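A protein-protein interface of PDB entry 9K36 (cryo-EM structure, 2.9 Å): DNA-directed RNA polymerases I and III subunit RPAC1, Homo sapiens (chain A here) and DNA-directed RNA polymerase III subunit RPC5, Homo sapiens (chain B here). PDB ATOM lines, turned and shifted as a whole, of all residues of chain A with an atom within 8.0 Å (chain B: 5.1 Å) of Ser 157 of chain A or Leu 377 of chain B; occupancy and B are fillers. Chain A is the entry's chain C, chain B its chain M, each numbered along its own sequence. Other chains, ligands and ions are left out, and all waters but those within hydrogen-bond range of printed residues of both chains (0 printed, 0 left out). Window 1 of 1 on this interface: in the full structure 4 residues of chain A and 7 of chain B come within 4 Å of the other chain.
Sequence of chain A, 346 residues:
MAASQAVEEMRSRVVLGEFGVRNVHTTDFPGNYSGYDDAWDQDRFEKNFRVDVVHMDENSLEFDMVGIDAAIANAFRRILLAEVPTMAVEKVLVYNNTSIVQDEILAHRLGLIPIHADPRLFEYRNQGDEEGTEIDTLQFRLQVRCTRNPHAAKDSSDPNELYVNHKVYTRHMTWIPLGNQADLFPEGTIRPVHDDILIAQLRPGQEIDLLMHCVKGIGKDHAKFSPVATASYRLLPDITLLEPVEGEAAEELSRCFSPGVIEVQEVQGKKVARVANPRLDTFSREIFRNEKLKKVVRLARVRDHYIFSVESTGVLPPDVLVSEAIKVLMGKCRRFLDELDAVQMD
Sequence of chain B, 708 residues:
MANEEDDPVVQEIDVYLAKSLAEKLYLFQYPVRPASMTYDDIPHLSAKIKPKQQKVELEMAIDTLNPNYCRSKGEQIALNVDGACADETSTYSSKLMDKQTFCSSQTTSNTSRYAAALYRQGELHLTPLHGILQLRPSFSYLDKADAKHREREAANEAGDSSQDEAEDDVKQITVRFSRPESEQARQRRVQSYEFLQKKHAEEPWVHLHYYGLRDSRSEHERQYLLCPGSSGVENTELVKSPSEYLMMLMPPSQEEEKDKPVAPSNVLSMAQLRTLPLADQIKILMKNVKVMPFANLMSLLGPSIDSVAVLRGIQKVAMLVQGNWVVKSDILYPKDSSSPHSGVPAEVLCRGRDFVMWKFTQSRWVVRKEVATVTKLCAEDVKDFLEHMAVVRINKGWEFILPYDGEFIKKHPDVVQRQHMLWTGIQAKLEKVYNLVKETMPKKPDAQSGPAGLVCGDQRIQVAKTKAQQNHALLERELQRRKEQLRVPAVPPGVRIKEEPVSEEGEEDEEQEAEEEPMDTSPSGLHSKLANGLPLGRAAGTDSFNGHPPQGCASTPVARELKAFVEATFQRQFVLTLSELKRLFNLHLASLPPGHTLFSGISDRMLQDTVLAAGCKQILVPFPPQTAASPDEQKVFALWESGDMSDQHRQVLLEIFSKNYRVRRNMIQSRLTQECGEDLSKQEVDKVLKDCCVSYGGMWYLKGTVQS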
ATOM      1  N   ALA A 153      -7.489 -15.385 -13.844  1.00  0.00           N
ATOM      2  CA  ALA A 153      -7.823 -16.462 -14.762  1.00  0.00           C
ATOM      3  C   ALA A 153      -6.899 -16.443 -15.975  1.00  0.00           C
ATOM      4  O   ALA A 153      -6.129 -15.501 -16.196  1.00  0.00           O
ATOM      5  CB  ALA A 153      -9.281 -16.356 -15.207  1.00  0.00           C
ATOM      6  N   LYS A 154      -6.981 -17.510 -16.773  1.00  0.00           N
ATOM      7  CA  LYS A 154      -6.141 -17.608 -17.964  1.00  0.00           C
ATOM      8  C   LYS A 154      -6.536 -16.566 -19.002  1.00  0.00           C
ATOM      9  O   LYS A 154      -5.670 -15.912 -19.597  1.00  0.00           O
ATOM     10  CB  LYS A 154      -6.231 -19.017 -18.551  1.00  0.00           C
ATOM     11  CG  LYS A 154      -5.929 -20.118 -17.549  1.00  0.00           C
ATOM     12  CD  LYS A 154      -4.549 -19.941 -16.933  1.00  0.00           C
ATOM     13  CE  LYS A 154      -4.282 -20.995 -15.871  1.00  0.00           C
ATOM     14  NZ  LYS A 154      -5.278 -20.926 -14.763  1.00  0.00           N
ATOM     15  N   ASP A 155      -7.838 -16.395 -19.234  1.00  0.00           N
ATOM     16  CA  ASP A 155      -8.300 -15.401 -20.198  1.00  0.00           C
ATOM     17  C   ASP A 155      -8.343 -14.010 -19.577  1.00  0.00           C
ATOM     18  O   ASP A 155      -7.611 -13.106 -20.000  1.00  0.00           O
ATOM     19  CB  ASP A 155      -9.677 -15.798 -20.736  1.00  0.00           C
ATOM     20  CG  ASP A 155     -10.618 -16.276 -19.643  1.00  0.00           C
ATOM     21  OD1 ASP A 155     -10.182 -16.357 -18.475  1.00  0.00           O
ATOM     22  OD2 ASP A 155     -11.791 -16.569 -19.951  1.00  0.00           O
ATOM     23  N   SER A 156      -9.181 -13.827 -18.555  1.00  0.00           N
ATOM     24  CA  SER A 156      -9.336 -12.557 -17.852  1.00  0.00           C
ATOM     25  C   SER A 156      -9.558 -11.403 -18.832  1.00  0.00           C
ATOM     26  O   SER A 156      -8.777 -10.453 -18.910  1.00  0.00           O
ATOM     27  CB  SER A 156      -8.132 -12.292 -16.944  1.00  0.00           C
ATOM     28  OG  SER A 156      -7.988 -13.316 -15.977  1.00  0.00           O
ATOM     29  N   SER A 157     -10.651 -11.508 -19.590  1.00  0.00           N
ATOM     30  CA  SER A 157     -10.956 -10.485 -20.586  1.00  0.00           C
ATOM     31  C   SER A 157     -11.309  -9.157 -19.924  1.00  0.00           C
ATOM     32  O   SER A 157     -10.963  -8.087 -20.438  1.00  0.00           O
ATOM     33  CB  SER A 157     -12.098 -10.953 -21.489  1.00  0.00           C
ATOM     34  OG  SER A 157     -12.416  -9.973 -22.460  1.00  0.00           O
ATOM     35  N   ASP A 158     -11.994  -9.206 -18.787  1.00  0.00           N
ATOM     36  CA  ASP A 158     -12.364  -7.982 -18.096  1.00  0.00           C
ATOM     37  C   ASP A 158     -11.135  -7.360 -17.435  1.00  0.00           C
ATOM     38  O   ASP A 158     -10.321  -8.073 -16.839  1.00  0.00           O
ATOM     39  CB  ASP A 158     -13.442  -8.262 -17.049  1.00  0.00           C
ATOM     40  CG  ASP A 158     -13.022  -9.321 -16.047  1.00  0.00           C
ATOM     41  OD1 ASP A 158     -12.257 -10.233 -16.427  1.00  0.00           O
ATOM     42  OD2 ASP A 158     -13.459  -9.240 -14.881  1.00  0.00           O
ATOM     43  N   PRO A 159     -10.967  -6.039 -17.531  1.00  0.00           N
ATOM     44  CA  PRO A 159      -9.802  -5.399 -16.897  1.00  0.00           C
ATOM     45  C   PRO A 159      -9.808  -5.482 -15.382  1.00  0.00           C
ATOM     46  O   PRO A 159      -8.753  -5.296 -14.764  1.00  0.00           O
ATOM     47  CB  PRO A 159      -9.894  -3.943 -17.377  1.00  0.00           C
ATOM     48  CG  PRO A 159     -10.788  -3.981 -18.580  1.00  0.00           C
ATOM     49  CD  PRO A 159     -11.764  -5.083 -18.317  1.00  0.00           C
ATOM     50  N   ASN A 160     -10.961  -5.747 -14.759  1.00  0.00           N
ATOM     51  CA  ASN A 160     -11.017  -5.821 -13.304  1.00  0.00           C
ATOM     52  C   ASN A 160     -10.207  -6.999 -12.775  1.00  0.00           C
ATOM     53  O   ASN A 160      -9.520  -6.880 -11.754  1.00  0.00           O
ATOM     54  CB  ASN A 160     -12.472  -5.919 -12.839  1.00  0.00           C
ATOM     55  CG  ASN A 160     -13.312  -4.748 -13.305  1.00  0.00           C
ATOM     56  OD1 ASN A 160     -14.257  -4.914 -14.075  1.00  0.00           O
ATOM     57  ND2 ASN A 160     -12.977  -3.552 -12.832  1.00  0.00           N
ATOM     58  N   GLU A 161     -10.275  -8.143 -13.456  1.00  0.00           N
ATOM     59  CA  GLU A 161      -9.552  -9.321 -12.990  1.00  0.00           C
ATOM     60  C   GLU A 161      -8.073  -9.248 -13.351  1.00  0.00           C
ATOM     61  O   GLU A 161      -7.217  -9.696 -12.579  1.00  0.00           O
ATOM     62  CB  GLU A 161     -10.185 -10.587 -13.571  1.00  0.00           C
ATOM     63  CG  GLU A 161      -9.637 -11.878 -12.991  1.00  0.00           C
ATOM     64  CD  GLU A 161     -10.350 -13.105 -13.524  1.00  0.00           C
ATOM     65  OE1 GLU A 161     -11.081 -12.982 -14.529  1.00  0.00           O
ATOM     66  OE2 GLU A 161     -10.181 -14.194 -12.935  1.00  0.00           O
ATOM     67  N   LEU A 162      -7.753  -8.684 -14.518  1.00  0.00           N
ATOM     68  CA  LEU A 162      -6.362  -8.638 -14.961  1.00  0.00           C
ATOM     69  C   LEU A 162      -5.536  -7.670 -14.123  1.00  0.00           C
ATOM     70  O   LEU A 162      -4.414  -7.993 -13.718  1.00  0.00           O
ATOM     71  CB  LEU A 162      -6.290  -8.249 -16.437  1.00  0.00           C
ATOM     72  CG  LEU A 162      -6.069  -9.378 -17.445  1.00  0.00           C
ATOM     73  CD1 LEU A 162      -5.920  -8.819 -18.852  1.00  0.00           C
ATOM     74  CD2 LEU A 162      -4.853 -10.208 -17.062  1.00  0.00           C
ATOM     75  N   TYR A 163      -6.065  -6.478 -13.859  1.00  0.00           N
ATOM     76  CA  TYR A 163      -5.305  -5.419 -13.215  1.00  0.00           C
ATOM     77  C   TYR A 163      -5.972  -5.001 -11.912  1.00  0.00           C
ATOM     78  O   TYR A 163      -7.166  -5.226 -11.696  1.00  0.00           O
ATOM     79  CB  TYR A 163      -5.164  -4.207 -14.144  1.00  0.00           C
ATOM     80  CG  TYR A 163      -5.023  -4.580 -15.602  1.00  0.00           C
ATOM     81  CD1 TYR A 163      -3.854  -5.155 -16.082  1.00  0.00           C
ATOM     82  CD2 TYR A 163      -6.059  -4.357 -16.498  1.00  0.00           C
ATOM     83  CE1 TYR A 163      -3.721  -5.500 -17.414  1.00  0.00           C
ATOM     84  CE2 TYR A 163      -5.936  -4.699 -17.832  1.00  0.00           C
ATOM     85  CZ  TYR A 163      -4.766  -5.269 -18.284  1.00  0.00           C
ATOM     86  OH  TYR A 163      -4.639  -5.611 -19.611  1.00  0.00           O
ATOM     87  N   SER B 342     -10.953  -7.665 -27.864  1.00  0.00           N
ATOM     88  CA  SER B 342     -10.104  -7.862 -26.699  1.00  0.00           C
ATOM     89  C   SER B 342      -8.791  -8.569 -26.995  1.00  0.00           C
ATOM     90  O   SER B 342      -7.852  -8.439 -26.200  1.00  0.00           O
ATOM     91  CB  SER B 342     -10.854  -8.659 -25.618  1.00  0.00           C
ATOM     92  OG  SER B 342     -11.236  -9.935 -26.098  1.00  0.00           O
ATOM     93  N   VAL B 344      -8.246 -11.822 -27.012  1.00  0.00           N
ATOM     94  CA  VAL B 344      -8.138 -13.092 -26.301  1.00  0.00           C
ATOM     95  C   VAL B 344      -8.045 -14.220 -27.325  1.00  0.00           C
ATOM     96  O   VAL B 344      -8.487 -14.047 -28.470  1.00  0.00           O
ATOM     97  CB  VAL B 344      -9.323 -13.296 -25.342  1.00  0.00           C
ATOM     98  CG1 VAL B 344      -9.376 -12.170 -24.319  1.00  0.00           C
ATOM     99  CG2 VAL B 344     -10.628 -13.380 -26.118  1.00  0.00           C
ATOM    100  N   VAL B 348     -11.002 -19.362 -25.920  1.00  0.00           N
ATOM    101  CA  VAL B 348     -11.885 -18.761 -24.925  1.00  0.00           C
ATOM    102  C   VAL B 348     -13.185 -18.305 -25.575  1.00  0.00           C
ATOM    103  O   VAL B 348     -14.268 -18.444 -24.992  1.00  0.00           O
ATOM    104  CB  VAL B 348     -11.170 -17.600 -24.213  1.00  0.00           C
ATOM    105  CG1 VAL B 348     -12.079 -16.987 -23.164  1.00  0.00           C
ATOM    106  CG2 VAL B 348      -9.874 -18.088 -23.586  1.00  0.00           C
ATOM    107  N   GLY B 352     -16.881 -19.631 -24.563  1.00  0.00           N
ATOM    108  CA  GLY B 352     -17.968 -18.726 -24.223  1.00  0.00           C
ATOM    109  C   GLY B 352     -19.182 -18.912 -25.111  1.00  0.00           C
ATOM    110  O   GLY B 352     -20.321 -18.900 -24.634  1.00  0.00           O
ATOM    111  N   ALA B 372     -21.778 -12.758 -18.569  1.00  0.00           N
ATOM    112  CA  ALA B 372     -20.562 -11.979 -18.367  1.00  0.00           C
ATOM    113  C   ALA B 372     -19.872 -12.360 -17.062  1.00  0.00           C
ATOM    114  O   ALA B 372     -18.637 -12.381 -16.986  1.00  0.00           O
ATOM    115  CB  ALA B 372     -20.884 -10.485 -18.388  1.00  0.00           C
ATOM    116  N   THR B 375     -18.564 -16.399 -17.638  1.00  0.00           N
ATOM    117  CA  THR B 375     -17.487 -16.533 -18.610  1.00  0.00           C
ATOM    118  C   THR B 375     -16.324 -15.584 -18.353  1.00  0.00           C
ATOM    119  O   THR B 375     -15.284 -15.721 -19.005  1.00  0.00           O
ATOM    120  CB  THR B 375     -18.021 -16.298 -20.026  1.00  0.00           C
ATOM    121  OG1 THR B 375     -18.578 -14.980 -20.112  1.00  0.00           O
ATOM    122  CG2 THR B 375     -19.094 -17.322 -20.367  1.00  0.00           C
ATOM    123  N   LYS B 376     -16.478 -14.631 -17.431  1.00  0.00           N
ATOM    124  CA  LYS B 376     -15.438 -13.659 -17.084  1.00  0.00           C
ATOM    125  C   LYS B 376     -14.974 -12.851 -18.291  1.00  0.00           C
ATOM    126  O   LYS B 376     -13.842 -12.359 -18.314  1.00  0.00           O
ATOM    127  CB  LYS B 376     -14.240 -14.341 -16.414  1.00  0.00           C
ATOM    128  CG  LYS B 376     -14.580 -15.095 -15.139  1.00  0.00           C
ATOM    129  CD  LYS B 376     -15.124 -14.159 -14.071  1.00  0.00           C
ATOM    130  CE  LYS B 376     -15.434 -14.909 -12.788  1.00  0.00           C
ATOM    131  NZ  LYS B 376     -15.946 -13.998 -11.728  1.00  0.00           N
ATOM    132  N   LEU B 377     -15.829 -12.702 -19.297  1.00  0.00           N
ATOM    133  CA  LEU B 377     -15.476 -11.984 -20.511  1.00  0.00           C
ATOM    134  C   LEU B 377     -15.951 -10.535 -20.446  1.00  0.00           C
ATOM    135  O   LEU B 377     -16.743 -10.150 -19.584  1.00  0.00           O
ATOM    136  CB  LEU B 377     -16.076 -12.677 -21.737  1.00  0.00           C
ATOM    137  CG  LEU B 377     -15.558 -14.085 -22.032  1.00  0.00           C
ATOM    138  CD1 LEU B 377     -16.233 -14.646 -23.273  1.00  0.00           C
ATOM    139  CD2 LEU B 377     -14.048 -14.077 -22.197  1.00  0.00           C
ATOM    140  N   CYS B 378     -15.444  -9.731 -21.377  1.00  0.00           N
ATOM    141  CA  CYS B 378     -15.836  -8.334 -21.453  1.00  0.00           C
ATOM    142  C   CYS B 378     -17.243  -8.202 -22.033  1.00  0.00           C
ATOM    143  O   CYS B 378     -17.836  -9.162 -22.530  1.00  0.00           O
ATOM    144  CB  CYS B 378     -14.839  -7.543 -22.296  1.00  0.00           C
ATOM    145  SG  CYS B 378     -14.513  -8.259 -23.919  1.00  0.00           S
ATOM    146  N   ALA B 379     -17.777  -6.978 -21.965  1.00  0.00           N
ATOM    147  CA  ALA B 379     -19.150  -6.744 -22.403  1.00  0.00           C
ATOM    148  C   ALA B 379     -19.291  -6.893 -23.914  1.00  0.00           C
ATOM    149  O   ALA B 379     -20.301  -7.417 -24.400  1.00  0.00           O
ATOM    150  CB  ALA B 379     -19.611  -5.356 -21.960  1.00  0.00           C
ATOM    151  N   ASP B 381     -17.581  -8.777 -26.096  1.00  0.00           N
ATOM    152  CA  ASP B 381     -17.555 -10.158 -26.573  1.00  0.00           C
ATOM    153  C   ASP B 381     -18.881 -10.859 -26.308  1.00  0.00           C
ATOM    154  O   ASP B 381     -19.398 -11.571 -27.178  1.00  0.00           O
ATOM    155  CB  ASP B 381     -16.403 -10.922 -25.923  1.00  0.00           C
ATOM    156  CG  ASP B 381     -15.053 -10.534 -26.491  1.00  0.00           C
ATOM    157  OD1 ASP B 381     -15.015  -9.985 -27.614  1.00  0.00           O
ATOM    158  OD2 ASP B 381     -14.029 -10.782 -25.822  1.00  0.00           O
ATOM    159  N   VAL B 382     -19.453 -10.666 -25.117  1.00  0.00           N
ATOM    160  CA  VAL B 382     -20.752 -11.259 -24.811  1.00  0.00           C
ATOM    161  C   VAL B 382     -21.827 -10.667 -25.712  1.00  0.00           C
ATOM    162  O   VAL B 382     -22.740 -11.370 -26.161  1.00  0.00           O
ATOM    163  CB  VAL B 382     -21.088 -11.068 -23.321  1.00  0.00           C
ATOM    164  CG1 VAL B 382     -22.432 -11.701 -22.988  1.00  0.00           C
ATOM    165  CG2 VAL B 382     -19.988 -11.658 -22.451  1.00  0.00           C
ATOM    166  N   PHE B 385     -21.500 -12.288 -29.049  1.00  0.00           N
ATOM    167  CA  PHE B 385     -21.995 -13.661 -28.964  1.00  0.00           C
ATOM    168  C   PHE B 385     -23.520 -13.700 -28.977  1.00  0.00           C
ATOM    169  O   PHE B 385     -24.118 -14.573 -29.615  1.00  0.00           O
ATOM    170  CB  PHE B 385     -21.457 -14.339 -27.704  1.00  0.00           C
ATOM    171  CG  PHE B 385     -19.980 -14.601 -27.736  1.00  0.00           C
ATOM    172  CD1 PHE B 385     -19.306 -14.704 -28.940  1.00  0.00           C
ATOM    173  CD2 PHE B 385     -19.264 -14.746 -26.558  1.00  0.00           C
ATOM    174  CE1 PHE B 385     -17.945 -14.947 -28.968  1.00  0.00           C
ATOM    175  CE2 PHE B 385     -17.904 -14.987 -26.581  1.00  0.00           C
ATOM    176  CZ  PHE B 385     -17.244 -15.089 -27.789  1.00  0.00           C
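Ser 157 of chain A touches five residues of chain B. Leu 377 of chain B touches just one residue of chain A: Ser 157. Of the printed residues of chain A, Cys 378 of chain B touches Ser 157 (3.1 Å). Printed residues of chain A within 4 Å of Ser 342 of chain B: Ser 157. Printed residues of chain A within 4 Å of Lys 376 of chain B: Ser 157 (3.5 Å), Asp 158 (3.3 Å) and Glu 161 (3.9 Å). Ala 153 of chain A touches none of the printed residues of chain B. The nearest residue of chain B that does not touch Ser 157 of chain A is Val 344 of chain B (4.1 Å). The nearest residue of chain A that does not touch Leu 377 of chain B is Asp 155 of chain A (4.04 Å).
Along chain A the printed residues that touch a printed residue of chain B span positions 155 to 161. Of the 13 printed residues of chain B, 7 touch a printed residue of chain A. Along chain B the printed residues that touch a printed residue of chain A span positions 342 to 381.
The side-chain sulfur of Cys 378 of chain B is in hydrogen-bond range of the side-chain hydroxyl of Ser 157 of chain A, 3.1 Å away. OD1 of Asp 158 of chain A sits close to O of Lys 376 of chain B (3.3 Å).
Among the printed residues, pairs that only touch across the chains: Asp 155 of chain A with Val 348 of chain B, Asp 155 of chain A with Thr 375 of chain B, Ser 157 of chain A with Ser 342 of chain B, Ser 157 of chain A with Lys 376 of chain B, Ser 157 of chain A with Leu 377 of chain B, Ser 157 of chain A with Asp 381 of chain B and Glu 161 of chain A with Lys 376 of chain B.
OE1 of Glu 161 of chain A lies close to OG of Ser 156 of chain A, at 3.4 Å. The backbone NH (N) of Ala 153 of chain A is in hydrogen-bond range of the side-chain carboxylate (OE2) of Glu 161 of chain A. SG of Cys 378 of chain B is in hydrogen-bond range of OD2 of Asp 381 of chain B. The side-chain hydroxyl (OG) of Ser 342 of chain B sits at hydrogen-bond distance from the side-chain carboxylate (OD2) of Asp 381 of chain B, 2.9 Å away.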
